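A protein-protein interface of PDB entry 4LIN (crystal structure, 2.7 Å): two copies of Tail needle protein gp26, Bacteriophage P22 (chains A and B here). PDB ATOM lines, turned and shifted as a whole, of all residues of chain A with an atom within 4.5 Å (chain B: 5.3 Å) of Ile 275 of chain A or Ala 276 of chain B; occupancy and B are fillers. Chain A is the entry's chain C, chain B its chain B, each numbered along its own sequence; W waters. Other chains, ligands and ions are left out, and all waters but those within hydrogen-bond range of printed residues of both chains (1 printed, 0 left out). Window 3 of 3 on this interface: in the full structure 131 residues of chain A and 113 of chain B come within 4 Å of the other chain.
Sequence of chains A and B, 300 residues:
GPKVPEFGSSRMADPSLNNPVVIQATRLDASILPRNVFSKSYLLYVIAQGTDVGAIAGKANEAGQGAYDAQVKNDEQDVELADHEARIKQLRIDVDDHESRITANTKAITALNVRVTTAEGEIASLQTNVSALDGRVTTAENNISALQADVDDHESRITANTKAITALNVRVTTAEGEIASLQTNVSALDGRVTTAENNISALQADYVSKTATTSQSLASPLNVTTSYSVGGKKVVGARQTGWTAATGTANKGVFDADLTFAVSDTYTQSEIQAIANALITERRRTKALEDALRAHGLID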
ATOM      1  N   THR A 260      -2.046  30.979   9.625  1.00  0.00           N
ATOM      2  CA  THR A 260      -0.949  30.528   8.805  1.00  0.00           C
ATOM      3  C   THR A 260      -1.203  31.336   7.553  1.00  0.00           C
ATOM      4  O   THR A 260      -2.124  31.046   6.786  1.00  0.00           O
ATOM      5  CB  THR A 260      -1.033  29.020   8.510  1.00  0.00           C
ATOM      6  OG1 THR A 260      -2.397  28.588   8.591  1.00  0.00           O
ATOM      7  CG2 THR A 260      -0.204  28.227   9.515  1.00  0.00           C
ATOM      8  N   GLU A 271       5.431  28.816   3.353  1.00  0.00           N
ATOM      9  CA  GLU A 271       4.148  28.753   4.049  1.00  0.00           C
ATOM     10  C   GLU A 271       3.624  27.334   4.243  1.00  0.00           C
ATOM     11  O   GLU A 271       3.180  26.976   5.335  1.00  0.00           O
ATOM     12  CB  GLU A 271       3.085  29.576   3.343  1.00  0.00           C
ATOM     13  CG  GLU A 271       1.708  29.248   3.871  1.00  0.00           C
ATOM     14  CD  GLU A 271       0.627  30.015   3.184  1.00  0.00           C
ATOM     15  OE1 GLU A 271      -0.029  29.452   2.286  1.00  0.00           O
ATOM     16  OE2 GLU A 271       0.435  31.181   3.561  1.00  0.00           O
ATOM     17  N   ILE A 272       3.658  26.533   3.182  1.00  0.00           N
ATOM     18  CA  ILE A 272       3.258  25.132   3.290  1.00  0.00           C
ATOM     19  C   ILE A 272       4.191  24.466   4.303  1.00  0.00           C
ATOM     20  O   ILE A 272       3.774  23.594   5.064  1.00  0.00           O
ATOM     21  CB  ILE A 272       3.264  24.405   1.922  1.00  0.00           C
ATOM     22  CG1 ILE A 272       1.990  24.709   1.134  1.00  0.00           C
ATOM     23  CG2 ILE A 272       3.354  22.908   2.103  1.00  0.00           C
ATOM     24  CD1 ILE A 272       1.881  26.122   0.604  1.00  0.00           C
ATOM     25  N   GLN A 273       5.441  24.923   4.332  1.00  0.00           N
ATOM     26  CA  GLN A 273       6.392  24.535   5.368  1.00  0.00           C
ATOM     27  C   GLN A 273       5.928  24.969   6.759  1.00  0.00           C
ATOM     28  O   GLN A 273       6.205  24.293   7.745  1.00  0.00           O
ATOM     29  CB  GLN A 273       7.776  25.124   5.083  1.00  0.00           C
ATOM     30  CG  GLN A 273       8.691  24.230   4.257  1.00  0.00           C
ATOM     31  CD  GLN A 273      10.143  24.668   4.327  1.00  0.00           C
ATOM     32  OE1 GLN A 273      10.441  25.825   4.624  1.00  0.00           O
ATOM     33  NE2 GLN A 273      11.054  23.741   4.059  1.00  0.00           N
ATOM     34  N   ALA A 274       5.242  26.104   6.841  1.00  0.00           N
ATOM     35  CA  ALA A 274       4.685  26.556   8.113  1.00  0.00           C
ATOM     36  C   ALA A 274       3.426  25.763   8.462  1.00  0.00           C
ATOM     37  O   ALA A 274       3.275  25.295   9.589  1.00  0.00           O
ATOM     38  CB  ALA A 274       4.385  28.046   8.073  1.00  0.00           C
ATOM     39  N   ILE A 275       2.532  25.617   7.486  1.00  0.00           N
ATOM     40  CA  ILE A 275       1.295  24.856   7.657  1.00  0.00           C
ATOM     41  C   ILE A 275       1.589  23.405   8.036  1.00  0.00           C
ATOM     42  O   ILE A 275       0.899  22.818   8.869  1.00  0.00           O
ATOM     43  CB  ILE A 275       0.416  24.910   6.382  1.00  0.00           C
ATOM     44  CG1 ILE A 275      -0.081  26.334   6.129  1.00  0.00           C
ATOM     45  CG2 ILE A 275      -0.765  23.954   6.489  1.00  0.00           C
ATOM     46  CD1 ILE A 275      -1.043  26.461   4.961  1.00  0.00           C
ATOM     47  N   ALA A 276       2.627  22.836   7.431  1.00  0.00           N
ATOM     48  CA  ALA A 276       3.059  21.486   7.773  1.00  0.00           C
ATOM     49  C   ALA A 276       3.726  21.451   9.149  1.00  0.00           C
ATOM     50  O   ALA A 276       3.727  20.416   9.812  1.00  0.00           O
ATOM     51  CB  ALA A 276       3.995  20.934   6.709  1.00  0.00           C
ATOM     52  N   ASN A 277       4.308  22.574   9.564  1.00  0.00           N
ATOM     53  CA  ASN A 277       4.875  22.689  10.907  1.00  0.00           C
ATOM     54  C   ASN A 277       3.865  23.196  11.948  1.00  0.00           C
ATOM     55  O   ASN A 277       4.125  23.139  13.147  1.00  0.00           O
ATOM     56  CB  ASN A 277       6.141  23.560  10.891  1.00  0.00           C
ATOM     57  CG  ASN A 277       7.305  22.898  10.166  1.00  0.00           C
ATOM     58  OD1 ASN A 277       7.175  21.802   9.621  1.00  0.00           O
ATOM     59  ND2 ASN A 277       8.449  23.576  10.145  1.00  0.00           N
ATOM     60  N   ALA A 278       2.727  23.707  11.481  1.00  0.00           N
ATOM     61  CA  ALA A 278       1.637  24.120  12.365  1.00  0.00           C
ATOM     62  C   ALA A 278       0.615  22.993  12.491  1.00  0.00           C
ATOM     63  O   ALA A 278      -0.350  23.089  13.249  1.00  0.00           O
ATOM     64  CB  ALA A 278       0.973  25.383  11.842  1.00  0.00           C
ATOM     65  N   LEU A 279       0.853  21.930  11.731  1.00  0.00           N
ATOM     66  CA  LEU A 279       0.075  20.697  11.787  1.00  0.00           C
ATOM     67  C   LEU A 279       0.739  19.758  12.784  1.00  0.00           C
ATOM     68  O   LEU A 279       0.095  19.271  13.714  1.00  0.00           O
ATOM     69  CB  LEU A 279      -0.046  20.036  10.412  1.00  0.00           C
ATOM     70  CG  LEU A 279      -1.117  18.946  10.318  1.00  0.00           C
ATOM     71  CD1 LEU A 279      -2.501  19.537  10.520  1.00  0.00           C
ATOM     72  CD2 LEU A 279      -1.040  18.196   8.995  1.00  0.00           C
ATOM     73  N   ILE B 272      -5.072  26.793  -0.485  1.00  0.00           N
ATOM     74  CA  ILE B 272      -4.137  26.493   0.585  1.00  0.00           C
ATOM     75  C   ILE B 272      -4.589  27.249   1.833  1.00  0.00           C
ATOM     76  O   ILE B 272      -4.356  26.809   2.960  1.00  0.00           O
ATOM     77  CB  ILE B 272      -2.695  26.901   0.194  1.00  0.00           C
ATOM     78  CG1 ILE B 272      -2.249  26.173  -1.078  1.00  0.00           C
ATOM     79  CG2 ILE B 272      -1.719  26.642   1.334  1.00  0.00           C
ATOM     80  CD1 ILE B 272      -2.122  24.668  -0.925  1.00  0.00           C
ATOM     81  N   GLN B 273      -5.256  28.381   1.621  1.00  0.00           N
ATOM     82  CA  GLN B 273      -5.820  29.158   2.719  1.00  0.00           C
ATOM     83  C   GLN B 273      -7.074  28.490   3.283  1.00  0.00           C
ATOM     84  O   GLN B 273      -7.524  28.827   4.373  1.00  0.00           O
ATOM     85  CB  GLN B 273      -6.115  30.598   2.284  1.00  0.00           C
ATOM     86  CG  GLN B 273      -7.108  30.732   1.137  1.00  0.00           C
ATOM     87  CD  GLN B 273      -7.083  32.113   0.506  1.00  0.00           C
ATOM     88  OE1 GLN B 273      -6.201  32.923   0.791  1.00  0.00           O
ATOM     89  NE2 GLN B 273      -8.052  32.387  -0.360  1.00  0.00           N
ATOM     90  N   ALA B 274      -7.631  27.540   2.538  1.00  0.00           N
ATOM     91  CA  ALA B 274      -8.753  26.746   3.029  1.00  0.00           C
ATOM     92  C   ALA B 274      -8.250  25.679   3.998  1.00  0.00           C
ATOM     93  O   ALA B 274      -8.931  25.330   4.960  1.00  0.00           O
ATOM     94  CB  ALA B 274      -9.504  26.109   1.877  1.00  0.00           C
ATOM     95  N   ILE B 275      -7.054  25.163   3.726  1.00  0.00           N
ATOM     96  CA  ILE B 275      -6.395  24.212   4.615  1.00  0.00           C
ATOM     97  C   ILE B 275      -5.770  24.968   5.787  1.00  0.00           C
ATOM     98  O   ILE B 275      -5.595  24.421   6.873  1.00  0.00           O
ATOM     99  CB  ILE B 275      -5.321  23.397   3.859  1.00  0.00           C
ATOM    100  CG1 ILE B 275      -5.898  22.845   2.554  1.00  0.00           C
ATOM    101  CG2 ILE B 275      -4.766  22.276   4.729  1.00  0.00           C
ATOM    102  CD1 ILE B 275      -4.967  21.949   1.765  1.00  0.00           C
ATOM    103  N   ALA B 276      -5.459  26.239   5.556  1.00  0.00           N
ATOM    104  CA  ALA B 276      -4.869  27.098   6.576  1.00  0.00           C
ATOM    105  C   ALA B 276      -5.925  27.601   7.557  1.00  0.00           C
ATOM    106  O   ALA B 276      -5.637  27.812   8.730  1.00  0.00           O
ATOM    107  CB  ALA B 276      -4.146  28.264   5.928  1.00  0.00           C
ATOM    108  N   ASN B 277      -7.140  27.817   7.058  1.00  0.00           N
ATOM    109  CA  ASN B 277      -8.243  28.261   7.900  1.00  0.00           C
ATOM    110  C   ASN B 277      -8.858  27.114   8.702  1.00  0.00           C
ATOM    111  O   ASN B 277      -9.497  27.339   9.727  1.00  0.00           O
ATOM    112  CB  ASN B 277      -9.318  28.969   7.066  1.00  0.00           C
ATOM    113  CG  ASN B 277      -8.836  30.289   6.483  1.00  0.00           C
ATOM    114  OD1 ASN B 277      -7.858  30.869   6.949  1.00  0.00           O
ATOM    115  ND2 ASN B 277      -9.528  30.767   5.451  1.00  0.00           N
ATOM    116  N   ALA B 278      -8.678  25.889   8.217  1.00  0.00           N
ATOM    117  CA  ALA B 278      -9.182  24.705   8.909  1.00  0.00           C
ATOM    118  C   ALA B 278      -8.180  24.129   9.909  1.00  0.00           C
ATOM    119  O   ALA B 278      -8.540  23.310  10.753  1.00  0.00           O
ATOM    120  CB  ALA B 278      -9.599  23.648   7.908  1.00  0.00           C
ATOM    121  N   LEU B 279      -6.923  24.548   9.808  1.00  0.00           N
ATOM    122  CA  LEU B 279      -5.920  24.178  10.799  1.00  0.00           C
ATOM    123  C   LEU B 279      -6.071  25.084  12.011  1.00  0.00           C
ATOM    124  O   LEU B 279      -5.867  24.661  13.148  1.00  0.00           O
ATOM    125  CB  LEU B 279      -4.503  24.284  10.223  1.00  0.00           C
ATOM    126  CG  LEU B 279      -3.334  24.042  11.184  1.00  0.00           C
ATOM    127  CD1 LEU B 279      -2.276  23.164  10.544  1.00  0.00           C
ATOM    128  CD2 LEU B 279      -2.713  25.356  11.640  1.00  0.00           C
ATOM    129  N   ILE B 280      -6.437  26.337  11.753  1.00  0.00           N
ATOM    130  CA  ILE B 280      -6.539  27.340  12.805  1.00  0.00           C
ATOM    131  C   ILE B 280      -7.914  27.427  13.472  1.00  0.00           C
ATOM    132  O   ILE B 280      -8.048  28.072  14.508  1.00  0.00           O
ATOM    133  CB  ILE B 280      -6.141  28.735  12.289  1.00  0.00           C
ATOM    134  CG1 ILE B 280      -7.177  29.246  11.289  1.00  0.00           C
ATOM    135  CG2 ILE B 280      -4.757  28.688  11.665  1.00  0.00           C
ATOM    136  CD1 ILE B 280      -7.003  30.700  10.923  1.00  0.00           C
HETATM  137  O   HOH W   1      -5.142  31.638   7.435  1.00  0.00           O
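The side-chain hydroxyl of Thr 260 of chain A lies close to the backbone carbonyl oxygen of Ala 276 of chain B, at 3.3 Å.
OG1 of Thr 260 of chain A touches CG2 of Ile 280 of chain B, 3.9 Å away. Ile 272 of chain B touches Glu 271 of chain A (CG2 to OE1, 3.4 Å). CD1 of Ile 272 of chain A touches CG2 of Ile 272 of chain B (3.7 Å). Ile 275 of chain A touches Ile 272 of chain B (CD1 to CG2, 3.7 Å). CD1 of Ile 275 of chain A touches CB of Ala 276 of chain B, at 3.7 Å. Ile 275 of chain A touches Leu 279 of chain B. O of Ala 278 of chain A touches CD1 of Leu 279 of chain B, at 3.3 Å. Leu 279 of chain B touches Leu 279 of chain A.
Of chain B, only Ile 272, Ala 276 and Leu 279 come within 4 Å of Ile 275 of chain A. Ala 276 of chain B touches two residues of chain A. Of the printed residues of chain B, Thr 260 of chain A touches Ala 276 (3.2 Å) and Ile 280 (3.9 Å). Printed residues of chain A within 4 Å of Ile 272 of chain B: Glu 271, Ile 272 and Ile 275. Printed residues of chain B within 4 Å of Ala 278 of chain A: Leu 279 (3.3 Å). The nearest printed residue of chain A that does not touch Ala 276 of chain B is Glu 271 of chain A (5.6 Å).
Printed residues of chain B that touch a printed residue of chain A: Ile 272, Ala 276, Leu 279 and Ile 280. Of the 10 printed residues of chain A, 6 touch a printed residue of chain B. Hydrophobic or aromatic side chains of chain A that line the printed part of chain B: Ile 272, Ile 275, Ala 278 and Leu 279. Among the printed residues, no Asp or Glu carboxylate lies within 4 Å of a Lys or Arg side-chain nitrogen of the other chain.
Ile 272 of chain A touches its own counterpart, Ile 272 of chain B. Ile 275 of chain A touches Ile 272 of chain B, but with the chains exchanged Ile 272 of chain A does not touch Ile 275 of chain B (7.5 Å). Ile 275 of chain A touches Ala 276 of chain B, but with the chains exchanged Ala 276 of chain A does not touch Ile 275 of chain B (7.9 Å). Ile 275 of chain A touches Leu 279 of chain B, but with the chains exchanged Leu 279 of chain A does not touch Ile 275 of chain B (6.8 Å). Of the 9 pairs that touch across the chains among the printed residues, 2 have their exchanged pair printed and touching as well.
Water W1 lies within hydrogen-bond range of the side-chain amide oxygen (OD1) of Asn 277 of chain B and the backbone carbonyl oxygen (O) of Thr 260 of chain A.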
